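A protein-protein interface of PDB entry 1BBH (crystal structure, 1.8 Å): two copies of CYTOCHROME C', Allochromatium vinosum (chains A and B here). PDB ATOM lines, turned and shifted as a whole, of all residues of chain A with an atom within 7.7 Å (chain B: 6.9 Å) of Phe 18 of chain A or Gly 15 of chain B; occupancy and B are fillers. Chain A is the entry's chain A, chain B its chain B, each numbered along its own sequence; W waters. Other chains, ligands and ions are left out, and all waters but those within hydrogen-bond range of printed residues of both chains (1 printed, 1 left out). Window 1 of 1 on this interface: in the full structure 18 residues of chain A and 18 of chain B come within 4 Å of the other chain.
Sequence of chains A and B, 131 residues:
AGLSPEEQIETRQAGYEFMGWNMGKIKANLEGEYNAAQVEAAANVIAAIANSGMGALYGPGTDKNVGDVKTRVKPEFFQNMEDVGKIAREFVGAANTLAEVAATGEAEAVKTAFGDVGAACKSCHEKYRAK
The side-chain carboxylate of Glu 17 of chain A sits close to the backbone NH of Thr 11 of chain B, 3.1 Å away. The backbone carbonyl oxygen (O) of Glu 10 of chain B sits close to the side-chain carboxylate (OE2) of Glu 17 of chain A, 2.8 Å away. NZ of Lys 25 of chain A lies within hydrogen-bond range of O of Ser 52 of chain B (2.8 Å).
The side-chain amino group (NZ) of Lys 25 of chain A lies within hydrogen-bond range of the side-chain amide oxygen (OD1) of Asn 22 of chain A (3.0 Å). O of Ile 49 of chain B is in hydrogen-bond range of OG of Ser 52 of chain B, at 2.7 Å. The guanidinium group (NH2) of Arg 12 of chain B sits at hydrogen-bond distance from the backbone carbonyl oxygen (O) of Leu 57 of chain B, 3.1 Å away. O of Phe 18 of chain A sits at hydrogen-bond distance from ND2 of Asn 22 of chain A (2.9 Å).
Among the printed residues, pairs that only touch across the chains: Ala 14 of chain A with Ala 14 of chain B (3.5 Å), Gly 15 of chain A with Phe 18 of chain B (3.5 Å), Glu 17 of chain A with Ala 14 of chain B (3.1 Å), Phe 18 of chain A with Thr 11 of chain B (3.6 Å), Phe 18 of chain A with Gly 15 of chain B (3.4 Å), Phe 18 of chain A with Ile 49 of chain B (3.8 Å), Phe 18 of chain A with Ser 52 of chain B (3.5 Å), Trp 21 of chain A with Thr 11 of chain B (3.5 Å), Trp 21 of chain A with Ser 52 of chain B (3.4 Å), Trp 21 of chain A with Gly 53 of chain B (3.6 Å), Trp 21 of chain A with Leu 57 of chain B (3.7 Å), Val 45 of chain A with Ala 48 of chain B (3.3 Å), Val 45 of chain A with Ser 52 of chain B (3.7 Å) and Ile 49 of chain A with Phe 18 of chain B (3.97 Å).
Phe 18 of chain A touches four residues of chain B. Of the printed residues of chain A, Glu 10 of chain B touches Glu 17. Of the printed residues of chain A, Thr 11 of chain B touches Glu 17, Phe 18 and Trp 21. Ala 14 of chain B touches just these residues of chain A: Ala 14 and Glu 17. Gly 15 of chain B touches just one residue of chain A: Phe 18. Printed residues of chain A within 4 Å of Ala 48 of chain B: Val 45. Ala 50 of chain B touches none of the printed residues of chain A. The nearest residue of chain B that does not touch Phe 18 of chain A is Met 54 of chain B (4.1 Å). The nearest printed residue of chain B that does not touch Ile 49 of chain A is Val 45 of chain B (4.5 Å).
Hydrophobic or aromatic side chains of chain A within 4 Å of the printed part of chain B: Ala 14, Phe 18, Trp 21, Val 45 and Ile 49. Of the 19 printed residues of chain B, 10 touch a printed residue of chain A. Printed residues of chain B that touch a printed residue of chain A: Glu 10, Thr 11, Ala 14, Gly 15, Phe 18, Ala 48, Ile 49, Ser 52, Gly 53 and Leu 57. Hydrophobic or aromatic side chains of chain B within 4 Å of the printed part of chain A: Ala 14, Phe 18, Ala 48, Ile 49 and Leu 57. Along chain B the printed residues that touch a printed residue of chain A span positions 10 to 57. Among the printed residues, 17 pairs touch across the chains. Among the printed residues, no Asp or Glu carboxylate lies within 4 Å of a Lys or Arg side-chain nitrogen of the other chain.
Ala 14 of chain A touches its own counterpart, Ala 14 of chain B. Gly 15 of chain A touches Phe 18 of chain B, and with the chains exchanged Phe 18 of chain A touches Gly 15 of chain B. Glu 17 of chain A touches Ala 14 of chain B, but with the chains exchanged Ala 14 of chain A does not touch Glu 17 of chain B (4.2 Å). Phe 18 of chain A touches Ile 49 of chain B, and with the chains exchanged Ile 49 of chain A touches Phe 18 of chain B. Of the 17 pairs that touch across the chains among the printed residues, 5 have their exchanged pair printed and touching as well.
Water W1 lies within hydrogen-bond range of the backbone carbonyl oxygen (O) of Ala 41 of chain A and the backbone carbonyl oxygen (O) of Ala 48 of chain B.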
ATOM      1  N   ARG A  12       0.078  16.580  -8.973  1.00  0.00           N
ATOM      2  CA  ARG A  12      -0.971  16.314  -7.963  1.00  0.00           C
ATOM      3  C   ARG A  12      -2.276  16.258  -8.762  1.00  0.00           C
ATOM      4  O   ARG A  12      -3.160  15.453  -8.487  1.00  0.00           O
ATOM      5  CB  ARG A  12      -1.004  17.487  -6.845  1.00  0.00           C
ATOM      6  CG  ARG A  12      -1.223  18.830  -7.528  1.00  0.00           C
ATOM      7  CD  ARG A  12      -1.676  19.998  -6.724  1.00  0.00           C
ATOM      8  NE  ARG A  12      -0.564  20.692  -6.212  1.00  0.00           N
ATOM      9  CZ  ARG A  12      -0.480  22.001  -5.955  1.00  0.00           C
ATOM     10  NH1 ARG A  12      -1.360  22.994  -6.188  1.00  0.00           N
ATOM     11  NH2 ARG A  12       0.677  22.308  -5.408  1.00  0.00           N
ATOM     12  N   GLN A  13      -2.415  17.067  -9.799  1.00  0.00           N
ATOM     13  CA  GLN A  13      -3.628  17.059 -10.580  1.00  0.00           C
ATOM     14  C   GLN A  13      -3.734  15.694 -11.275  1.00  0.00           C
ATOM     15  O   GLN A  13      -4.810  15.128 -11.288  1.00  0.00           O
ATOM     16  CB  GLN A  13      -3.586  18.186 -11.590  1.00  0.00           C
ATOM     17  CG  GLN A  13      -3.833  19.570 -10.919  1.00  0.00           C
ATOM     18  CD  GLN A  13      -3.653  20.735 -11.856  1.00  0.00           C
ATOM     19  OE1 GLN A  13      -3.122  20.578 -12.954  1.00  0.00           O
ATOM     20  NE2 GLN A  13      -3.987  21.978 -11.566  1.00  0.00           N
ATOM     21  N   ALA A  14      -2.655  15.100 -11.758  1.00  0.00           N
ATOM     22  CA  ALA A  14      -2.677  13.773 -12.374  1.00  0.00           C
ATOM     23  C   ALA A  14      -3.151  12.760 -11.367  1.00  0.00           C
ATOM     24  O   ALA A  14      -4.010  11.940 -11.627  1.00  0.00           O
ATOM     25  CB  ALA A  14      -1.255  13.441 -12.808  1.00  0.00           C
ATOM     26  N   GLY A  15      -2.667  12.841 -10.126  1.00  0.00           N
ATOM     27  CA  GLY A  15      -3.033  11.883  -9.096  1.00  0.00           C
ATOM     28  C   GLY A  15      -4.498  11.935  -8.756  1.00  0.00           C
ATOM     29  O   GLY A  15      -5.151  10.894  -8.634  1.00  0.00           O
ATOM     30  N   TYR A  16      -5.009  13.156  -8.641  1.00  0.00           N
ATOM     31  CA  TYR A  16      -6.422  13.357  -8.376  1.00  0.00           C
ATOM     32  C   TYR A  16      -7.320  12.874  -9.515  1.00  0.00           C
ATOM     33  O   TYR A  16      -8.354  12.247  -9.298  1.00  0.00           O
ATOM     34  CB  TYR A  16      -6.747  14.835  -8.157  1.00  0.00           C
ATOM     35  CG  TYR A  16      -6.215  15.378  -6.827  1.00  0.00           C
ATOM     36  CD1 TYR A  16      -6.408  14.622  -5.662  1.00  0.00           C
ATOM     37  CD2 TYR A  16      -5.505  16.584  -6.785  1.00  0.00           C
ATOM     38  CE1 TYR A  16      -5.881  15.053  -4.427  1.00  0.00           C
ATOM     39  CE2 TYR A  16      -4.984  17.019  -5.568  1.00  0.00           C
ATOM     40  CZ  TYR A  16      -5.188  16.250  -4.439  1.00  0.00           C
ATOM     41  OH  TYR A  16      -4.623  16.763  -3.306  1.00  0.00           O
ATOM     42  N   GLU A  17      -6.931  13.191 -10.711  1.00  0.00           N
ATOM     43  CA  GLU A  17      -7.657  12.783 -11.914  1.00  0.00           C
ATOM     44  C   GLU A  17      -7.720  11.271 -12.071  1.00  0.00           C
ATOM     45  O   GLU A  17      -8.799  10.698 -12.311  1.00  0.00           O
ATOM     46  CB  GLU A  17      -6.972  13.395 -13.059  1.00  0.00           C
ATOM     47  CG  GLU A  17      -7.760  13.166 -14.365  1.00  0.00           C
ATOM     48  CD  GLU A  17      -7.139  12.032 -15.143  1.00  0.00           C
ATOM     49  OE1 GLU A  17      -7.241  10.833 -14.752  1.00  0.00           O
ATOM     50  OE2 GLU A  17      -6.647  12.309 -16.259  1.00  0.00           O
ATOM     51  N   PHE A  18      -6.606  10.567 -11.768  1.00  0.00           N
ATOM     52  CA  PHE A  18      -6.561   9.108 -11.873  1.00  0.00           C
ATOM     53  C   PHE A  18      -7.454   8.485 -10.827  1.00  0.00           C
ATOM     54  O   PHE A  18      -8.188   7.499 -11.111  1.00  0.00           O
ATOM     55  CB  PHE A  18      -5.125   8.548 -11.678  1.00  0.00           C
ATOM     56  CG  PHE A  18      -4.992   7.194 -12.422  1.00  0.00           C
ATOM     57  CD1 PHE A  18      -5.009   7.173 -13.794  1.00  0.00           C
ATOM     58  CD2 PHE A  18      -4.875   6.021 -11.709  1.00  0.00           C
ATOM     59  CE1 PHE A  18      -4.911   5.947 -14.447  1.00  0.00           C
ATOM     60  CE2 PHE A  18      -4.774   4.800 -12.344  1.00  0.00           C
ATOM     61  CZ  PHE A  18      -4.793   4.793 -13.714  1.00  0.00           C
ATOM     62  N   MET A  19      -7.494   9.093  -9.608  1.00  0.00           N
ATOM     63  CA  MET A  19      -8.436   8.605  -8.601  1.00  0.00           C
ATOM     64  C   MET A  19      -9.870   8.796  -9.049  1.00  0.00           C
ATOM     65  O   MET A  19     -10.690   7.893  -8.846  1.00  0.00           O
ATOM     66  CB  MET A  19      -8.298   9.319  -7.221  1.00  0.00           C
ATOM     67  CG  MET A  19      -7.010   8.871  -6.541  1.00  0.00           C
ATOM     68  SD  MET A  19      -7.023   9.248  -4.748  1.00  0.00           S
ATOM     69  CE  MET A  19      -6.781  10.996  -4.844  1.00  0.00           C
ATOM     70  N   GLY A  20     -10.179   9.897  -9.695  1.00  0.00           N
ATOM     71  CA  GLY A  20     -11.508  10.140 -10.204  1.00  0.00           C
ATOM     72  C   GLY A  20     -11.938   9.029 -11.190  1.00  0.00           C
ATOM     73  O   GLY A  20     -13.057   8.514 -11.076  1.00  0.00           O
ATOM     74  N   TRP A  21     -11.069   8.590 -12.109  1.00  0.00           N
ATOM     75  CA  TRP A  21     -11.420   7.519 -13.076  1.00  0.00           C
ATOM     76  C   TRP A  21     -11.778   6.252 -12.318  1.00  0.00           C
ATOM     77  O   TRP A  21     -12.832   5.627 -12.536  1.00  0.00           O
ATOM     78  CB  TRP A  21     -10.234   7.223 -14.016  1.00  0.00           C
ATOM     79  CG  TRP A  21     -10.440   6.030 -14.992  1.00  0.00           C
ATOM     80  CD1 TRP A  21     -11.565   5.908 -15.774  1.00  0.00           C
ATOM     81  CD2 TRP A  21      -9.569   4.981 -15.154  1.00  0.00           C
ATOM     82  NE1 TRP A  21     -11.420   4.781 -16.428  1.00  0.00           N
ATOM     83  CE2 TRP A  21     -10.252   4.205 -16.091  1.00  0.00           C
ATOM     84  CE3 TRP A  21      -8.357   4.541 -14.622  1.00  0.00           C
ATOM     85  CZ2 TRP A  21      -9.708   2.981 -16.483  1.00  0.00           C
ATOM     86  CZ3 TRP A  21      -7.809   3.326 -15.015  1.00  0.00           C
ATOM     87  CH2 TRP A  21      -8.492   2.553 -15.948  1.00  0.00           C
ATOM     88  N   ASN A  22     -10.943   5.918 -11.332  1.00  0.00           N
ATOM     89  CA  ASN A  22     -11.208   4.732 -10.546  1.00  0.00           C
ATOM     90  C   ASN A  22     -12.452   4.876  -9.697  1.00  0.00           C
ATOM     91  O   ASN A  22     -13.165   3.884  -9.546  1.00  0.00           O
ATOM     92  CB  ASN A  22      -9.993   4.406  -9.688  1.00  0.00           C
ATOM     93  CG  ASN A  22      -9.005   3.800 -10.674  1.00  0.00           C
ATOM     94  OD1 ASN A  22      -9.094   2.640 -11.050  1.00  0.00           O
ATOM     95  ND2 ASN A  22      -8.075   4.585 -11.187  1.00  0.00           N
ATOM     96  N   MET A  23     -12.799   6.091  -9.233  1.00  0.00           N
ATOM     97  CA  MET A  23     -14.009   6.285  -8.476  1.00  0.00           C
ATOM     98  C   MET A  23     -15.196   6.010  -9.401  1.00  0.00           C
ATOM     99  O   MET A  23     -16.117   5.244  -9.067  1.00  0.00           O
ATOM    100  CB  MET A  23     -14.065   7.710  -7.939  1.00  0.00           C
ATOM    101  CG  MET A  23     -13.289   8.001  -6.662  1.00  0.00           C
ATOM    102  SD  MET A  23     -13.697   7.033  -5.209  1.00  0.00           S
ATOM    103  CE  MET A  23     -14.962   8.128  -4.609  1.00  0.00           C
ATOM    104  N   GLY A  24     -15.161   6.545 -10.600  1.00  0.00           N
ATOM    105  CA  GLY A  24     -16.242   6.352 -11.567  1.00  0.00           C
ATOM    106  C   GLY A  24     -16.431   4.885 -11.925  1.00  0.00           C
ATOM    107  O   GLY A  24     -17.566   4.403 -12.089  1.00  0.00           O
ATOM    108  N   LYS A  25     -15.341   4.127 -12.006  1.00  0.00           N
ATOM    109  CA  LYS A  25     -15.464   2.690 -12.290  1.00  0.00           C
ATOM    110  C   LYS A  25     -16.127   1.947 -11.140  1.00  0.00           C
ATOM    111  O   LYS A  25     -16.896   1.007 -11.377  1.00  0.00           O
ATOM    112  CB  LYS A  25     -14.070   2.001 -12.579  1.00  0.00           C
ATOM    113  CG  LYS A  25     -13.403   2.346 -13.906  1.00  0.00           C
ATOM    114  CD  LYS A  25     -12.190   1.434 -14.184  1.00  0.00           C
ATOM    115  CE  LYS A  25     -11.147   1.630 -13.120  1.00  0.00           C
ATOM    116  NZ  LYS A  25      -9.861   1.036 -13.483  1.00  0.00           N
ATOM    117  N   ALA A  41      -9.457  -3.842  -8.015  1.00  0.00           N
ATOM    118  CA  ALA A  41      -8.324  -3.182  -8.592  1.00  0.00           C
ATOM    119  C   ALA A  41      -8.455  -1.648  -8.543  1.00  0.00           C
ATOM    120  O   ALA A  41      -7.466  -0.895  -8.401  1.00  0.00           O
ATOM    121  CB  ALA A  41      -8.183  -3.664 -10.031  1.00  0.00           C
ATOM    122  N   ALA A  42      -9.706  -1.162  -8.665  1.00  0.00           N
ATOM    123  CA  ALA A  42      -9.921   0.292  -8.681  1.00  0.00           C
ATOM    124  C   ALA A  42      -9.753   0.830  -7.239  1.00  0.00           C
ATOM    125  O   ALA A  42      -9.091   1.833  -6.986  1.00  0.00           O
ATOM    126  CB  ALA A  42     -11.330   0.587  -9.182  1.00  0.00           C
ATOM    127  N   VAL A  45      -6.266   1.208  -6.286  1.00  0.00           N
ATOM    128  CA  VAL A  45      -5.560   2.374  -6.763  1.00  0.00           C
ATOM    129  C   VAL A  45      -5.863   3.541  -5.820  1.00  0.00           C
ATOM    130  O   VAL A  45      -4.989   4.342  -5.537  1.00  0.00           O
ATOM    131  CB  VAL A  45      -5.996   2.697  -8.197  1.00  0.00           C
ATOM    132  CG1 VAL A  45      -5.489   4.047  -8.673  1.00  0.00           C
ATOM    133  CG2 VAL A  45      -5.466   1.565  -9.086  1.00  0.00           C
ATOM    134  N   ILE A  46      -7.066   3.658  -5.300  1.00  0.00           N
ATOM    135  CA  ILE A  46      -7.383   4.839  -4.482  1.00  0.00           C
ATOM    136  C   ILE A  46      -6.612   4.808  -3.142  1.00  0.00           C
ATOM    137  O   ILE A  46      -6.039   5.843  -2.700  1.00  0.00           O
ATOM    138  CB  ILE A  46      -8.942   4.899  -4.312  1.00  0.00           C
ATOM    139  CG1 ILE A  46      -9.612   5.255  -5.685  1.00  0.00           C
ATOM    140  CG2 ILE A  46      -9.321   6.004  -3.279  1.00  0.00           C
ATOM    141  CD1 ILE A  46     -11.060   4.715  -5.687  1.00  0.00           C
ATOM    142  N   ILE A  49      -2.915   5.701  -3.942  1.00  0.00           N
ATOM    143  CA  ILE A  49      -2.652   7.111  -4.136  1.00  0.00           C
ATOM    144  C   ILE A  49      -2.910   7.891  -2.837  1.00  0.00           C
ATOM    145  O   ILE A  49      -2.122   8.802  -2.511  1.00  0.00           O
ATOM    146  CB  ILE A  49      -3.493   7.609  -5.284  1.00  0.00           C
ATOM    147  CG1 ILE A  49      -2.964   6.833  -6.524  1.00  0.00           C
ATOM    148  CG2 ILE A  49      -3.382   9.144  -5.451  1.00  0.00           C
ATOM    149  CD1 ILE A  49      -3.695   7.289  -7.767  1.00  0.00           C
ATOM    150  N   GLU B  10      -6.650  11.952 -21.519  1.00  0.00           N
ATOM    151  CA  GLU B  10      -6.322  12.707 -20.283  1.00  0.00           C
ATOM    152  C   GLU B  10      -6.053  11.726 -19.159  1.00  0.00           C
ATOM    153  O   GLU B  10      -5.036  11.853 -18.480  1.00  0.00           O
ATOM    154  CB  GLU B  10      -7.485  13.640 -19.893  1.00  0.00           C
ATOM    155  CG  GLU B  10      -7.451  14.819 -20.851  1.00  0.00           C
ATOM    156  CD  GLU B  10      -8.550  15.884 -20.717  1.00  0.00           C
ATOM    157  OE1 GLU B  10      -9.562  15.644 -20.057  1.00  0.00           O
ATOM    158  OE2 GLU B  10      -8.386  16.958 -21.302  1.00  0.00           O
ATOM    159  N   THR B  11      -6.892  10.697 -18.922  1.00  0.00           N
ATOM    160  CA  THR B  11      -6.631   9.735 -17.882  1.00  0.00           C
ATOM    161  C   THR B  11      -5.411   8.875 -18.111  1.00  0.00           C
ATOM    162  O   THR B  11      -4.693   8.631 -17.116  1.00  0.00           O
ATOM    163  CB  THR B  11      -7.845   8.801 -17.699  1.00  0.00           C
ATOM    164  OG1 THR B  11      -8.962   9.698 -17.606  1.00  0.00           O
ATOM    165  CG2 THR B  11      -7.793   7.938 -16.390  1.00  0.00           C
ATOM    166  N   ARG B  12      -5.096   8.452 -19.346  1.00  0.00           N
ATOM    167  CA  ARG B  12      -3.947   7.537 -19.441  1.00  0.00           C
ATOM    168  C   ARG B  12      -2.686   8.327 -19.165  1.00  0.00           C
ATOM    169  O   ARG B  12      -1.819   7.882 -18.425  1.00  0.00           O
ATOM    170  CB  ARG B  12      -3.865   6.834 -20.851  1.00  0.00           C
ATOM    171  CG  ARG B  12      -3.652   7.796 -21.967  1.00  0.00           C
ATOM    172  CD  ARG B  12      -3.201   7.257 -23.291  1.00  0.00           C
ATOM    173  NE  ARG B  12      -4.296   6.977 -24.136  1.00  0.00           N
ATOM    174  CZ  ARG B  12      -4.444   7.247 -25.454  1.00  0.00           C
ATOM    175  NH1 ARG B  12      -3.718   7.910 -26.374  1.00  0.00           N
ATOM    176  NH2 ARG B  12      -5.548   6.764 -25.913  1.00  0.00           N
ATOM    177  N   GLN B  13      -2.628   9.551 -19.663  1.00  0.00           N
ATOM    178  CA  GLN B  13      -1.484  10.438 -19.402  1.00  0.00           C
ATOM    179  C   GLN B  13      -1.372  10.710 -17.880  1.00  0.00           C
ATOM    180  O   GLN B  13      -0.262  10.644 -17.344  1.00  0.00           O
ATOM    181  CB  GLN B  13      -1.668  11.755 -20.137  1.00  0.00           C
ATOM    182  CG  GLN B  13      -1.478  11.606 -21.620  1.00  0.00           C
ATOM    183  CD  GLN B  13      -1.848  12.833 -22.394  1.00  0.00           C
ATOM    184  OE1 GLN B  13      -2.492  13.774 -21.900  1.00  0.00           O
ATOM    185  NE2 GLN B  13      -1.424  12.871 -23.645  1.00  0.00           N
ATOM    186  N   ALA B  14      -2.513  10.932 -17.164  1.00  0.00           N
ATOM    187  CA  ALA B  14      -2.488  11.184 -15.719  1.00  0.00           C
ATOM    188  C   ALA B  14      -1.942   9.989 -14.986  1.00  0.00           C
ATOM    189  O   ALA B  14      -1.038  10.175 -14.155  1.00  0.00           O
ATOM    190  CB  ALA B  14      -3.874  11.473 -15.224  1.00  0.00           C
ATOM    191  N   GLY B  15      -2.318   8.737 -15.350  1.00  0.00           N
ATOM    192  CA  GLY B  15      -1.757   7.531 -14.729  1.00  0.00           C
ATOM    193  C   GLY B  15      -0.242   7.433 -14.951  1.00  0.00           C
ATOM    194  O   GLY B  15       0.539   7.172 -14.028  1.00  0.00           O
ATOM    195  N   TYR B  16       0.203   7.712 -16.172  1.00  0.00           N
ATOM    196  CA  TYR B  16       1.629   7.601 -16.489  1.00  0.00           C
ATOM    197  C   TYR B  16       2.499   8.622 -15.762  1.00  0.00           C
ATOM    198  O   TYR B  16       3.598   8.330 -15.322  1.00  0.00           O
ATOM    199  CB  TYR B  16       1.830   7.780 -18.006  1.00  0.00           C
ATOM    200  CG  TYR B  16       1.334   6.598 -18.862  1.00  0.00           C
ATOM    201  CD1 TYR B  16       1.665   5.296 -18.483  1.00  0.00           C
ATOM    202  CD2 TYR B  16       0.594   6.813 -20.021  1.00  0.00           C
ATOM    203  CE1 TYR B  16       1.270   4.187 -19.253  1.00  0.00           C
ATOM    204  CE2 TYR B  16       0.190   5.731 -20.797  1.00  0.00           C
ATOM    205  CZ  TYR B  16       0.542   4.441 -20.394  1.00  0.00           C
ATOM    206  OH  TYR B  16       0.161   3.339 -21.129  1.00  0.00           O
ATOM    207  N   GLU B  17       2.024   9.852 -15.712  1.00  0.00           N
ATOM    208  CA  GLU B  17       2.681  10.995 -15.066  1.00  0.00           C
ATOM    209  C   GLU B  17       2.734  10.698 -13.596  1.00  0.00           C
ATOM    210  O   GLU B  17       3.812  10.860 -13.013  1.00  0.00           O
ATOM    211  CB  GLU B  17       1.849  12.210 -15.388  1.00  0.00           C
ATOM    212  CG  GLU B  17       2.607  13.519 -15.346  1.00  0.00           C
ATOM    213  CD  GLU B  17       3.794  13.699 -16.300  1.00  0.00           C
ATOM    214  OE1 GLU B  17       3.671  13.612 -17.530  1.00  0.00           O
ATOM    215  OE2 GLU B  17       4.870  14.001 -15.798  1.00  0.00           O
ATOM    216  N   PHE B  18       1.675  10.124 -12.980  1.00  0.00           N
ATOM    217  CA  PHE B  18       1.743   9.834 -11.571  1.00  0.00           C
ATOM    218  C   PHE B  18       2.659   8.669 -11.308  1.00  0.00           C
ATOM    219  O   PHE B  18       3.344   8.656 -10.273  1.00  0.00           O
ATOM    220  CB  PHE B  18       0.370   9.540 -10.995  1.00  0.00           C
ATOM    221  CG  PHE B  18       0.346   9.858  -9.491  1.00  0.00           C
ATOM    222  CD1 PHE B  18       0.429  11.187  -9.098  1.00  0.00           C
ATOM    223  CD2 PHE B  18       0.223   8.850  -8.543  1.00  0.00           C
ATOM    224  CE1 PHE B  18       0.381  11.500  -7.743  1.00  0.00           C
ATOM    225  CE2 PHE B  18       0.176   9.172  -7.204  1.00  0.00           C
ATOM    226  CZ  PHE B  18       0.254  10.498  -6.798  1.00  0.00           C
ATOM    227  N   MET B  19       2.744   7.644 -12.206  1.00  0.00           N
ATOM    228  CA  MET B  19       3.741   6.559 -12.010  1.00  0.00           C
ATOM    229  C   MET B  19       5.191   7.097 -12.158  1.00  0.00           C
ATOM    230  O   MET B  19       6.058   6.675 -11.398  1.00  0.00           O
ATOM    231  CB  MET B  19       3.579   5.409 -13.042  1.00  0.00           C
ATOM    232  CG  MET B  19       2.410   4.514 -12.711  1.00  0.00           C
ATOM    233  SD  MET B  19       2.506   2.946 -13.651  1.00  0.00           S
ATOM    234  CE  MET B  19       2.141   3.602 -15.243  1.00  0.00           C
ATOM    235  N   GLY B  20       5.448   8.039 -13.074  1.00  0.00           N
ATOM    236  CA  GLY B  20       6.741   8.661 -13.219  1.00  0.00           C
ATOM    237  C   GLY B  20       7.177   9.386 -11.952  1.00  0.00           C
ATOM    238  O   GLY B  20       8.345   9.289 -11.559  1.00  0.00           O
ATOM    239  N   VAL B  45       2.031   2.201  -5.523  1.00  0.00           N
ATOM    240  CA  VAL B  45       1.355   3.018  -6.517  1.00  0.00           C
ATOM    241  C   VAL B  45       1.637   2.447  -7.916  1.00  0.00           C
ATOM    242  O   VAL B  45       0.717   2.272  -8.745  1.00  0.00           O
ATOM    243  CB  VAL B  45       1.839   4.510  -6.460  1.00  0.00           C
ATOM    244  CG1 VAL B  45       1.207   5.282  -7.614  1.00  0.00           C
ATOM    245  CG2 VAL B  45       1.443   5.176  -5.118  1.00  0.00           C
ATOM    246  N   ALA B  48      -0.361  -0.847  -8.293  1.00  0.00           N
ATOM    247  CA  ALA B  48      -1.800  -0.580  -8.382  1.00  0.00           C
ATOM    248  C   ALA B  48      -2.157   0.036  -9.723  1.00  0.00           C
ATOM    249  O   ALA B  48      -3.144  -0.422 -10.344  1.00  0.00           O
ATOM    250  CB  ALA B  48      -2.269   0.404  -7.290  1.00  0.00           C
ATOM    251  N   ILE B  49      -1.382   1.011 -10.262  1.00  0.00           N
ATOM    252  CA  ILE B  49      -1.724   1.619 -11.550  1.00  0.00           C
ATOM    253  C   ILE B  49      -1.389   0.625 -12.657  1.00  0.00           C
ATOM    254  O   ILE B  49      -2.196   0.509 -13.594  1.00  0.00           O
ATOM    255  CB  ILE B  49      -0.972   2.919 -11.787  1.00  0.00           C
ATOM    256  CG1 ILE B  49      -1.410   3.915 -10.643  1.00  0.00           C
ATOM    257  CG2 ILE B  49      -1.229   3.437 -13.233  1.00  0.00           C
ATOM    258  CD1 ILE B  49      -0.834   5.318 -10.776  1.00  0.00           C
ATOM    259  N   ALA B  50      -0.334  -0.189 -12.523  1.00  0.00           N
ATOM    260  CA  ALA B  50      -0.057  -1.241 -13.543  1.00  0.00           C
ATOM    261  C   ALA B  50      -1.259  -2.217 -13.602  1.00  0.00           C
ATOM    262  O   ALA B  50      -1.711  -2.610 -14.680  1.00  0.00           O
ATOM    263  CB  ALA B  50       1.152  -2.073 -13.167  1.00  0.00           C
ATOM    264  N   SER B  52      -4.408  -1.544 -13.020  1.00  0.00           N
ATOM    265  CA  SER B  52      -5.709  -0.871 -13.033  1.00  0.00           C
ATOM    266  C   SER B  52      -6.578  -0.962 -14.282  1.00  0.00           C
ATOM    267  O   SER B  52      -7.690  -0.395 -14.404  1.00  0.00           O
ATOM    268  CB  SER B  52      -5.441   0.586 -12.666  1.00  0.00           C
ATOM    269  OG  SER B  52      -4.720   1.342 -13.614  1.00  0.00           O
ATOM    270  N   GLY B  53      -6.023  -1.712 -15.242  1.00  0.00           N
ATOM    271  CA  GLY B  53      -6.711  -1.938 -16.500  1.00  0.00           C
ATOM    272  C   GLY B  53      -6.637  -0.709 -17.375  1.00  0.00           C
ATOM    273  O   GLY B  53      -7.622  -0.316 -18.020  1.00  0.00           O
ATOM    274  N   MET B  54      -5.434  -0.118 -17.517  1.00  0.00           N
ATOM    275  CA  MET B  54      -5.270   1.022 -18.432  1.00  0.00           C
ATOM    276  C   MET B  54      -5.391   0.627 -19.883  1.00  0.00           C
ATOM    277  O   MET B  54      -5.473   1.537 -20.715  1.00  0.00           O
ATOM    278  CB  MET B  54      -3.916   1.682 -18.230  1.00  0.00           C
ATOM    279  CG  MET B  54      -3.809   2.412 -16.928  1.00  0.00           C
ATOM    280  SD  MET B  54      -2.150   3.116 -16.684  1.00  0.00           S
ATOM    281  CE  MET B  54      -2.159   4.475 -17.787  1.00  0.00           C
ATOM    282  N   LEU B  57      -8.049   2.371 -21.772  1.00  0.00           N
ATOM    283  CA  LEU B  57      -8.015   3.752 -22.149  1.00  0.00           C
ATOM    284  C   LEU B  57      -7.462   3.916 -23.545  1.00  0.00           C
ATOM    285  O   LEU B  57      -7.052   5.017 -23.891  1.00  0.00           O
ATOM    286  CB  LEU B  57      -7.173   4.533 -21.116  1.00  0.00           C
ATOM    287  CG  LEU B  57      -7.656   4.418 -19.653  1.00  0.00           C
ATOM    288  CD1 LEU B  57      -6.589   4.995 -18.727  1.00  0.00           C
ATOM    289  CD2 LEU B  57      -8.977   5.188 -19.456  1.00  0.00           C
HETATM  290  O   HOH W   1      -5.047  -1.914  -9.000  1.00  0.00           O
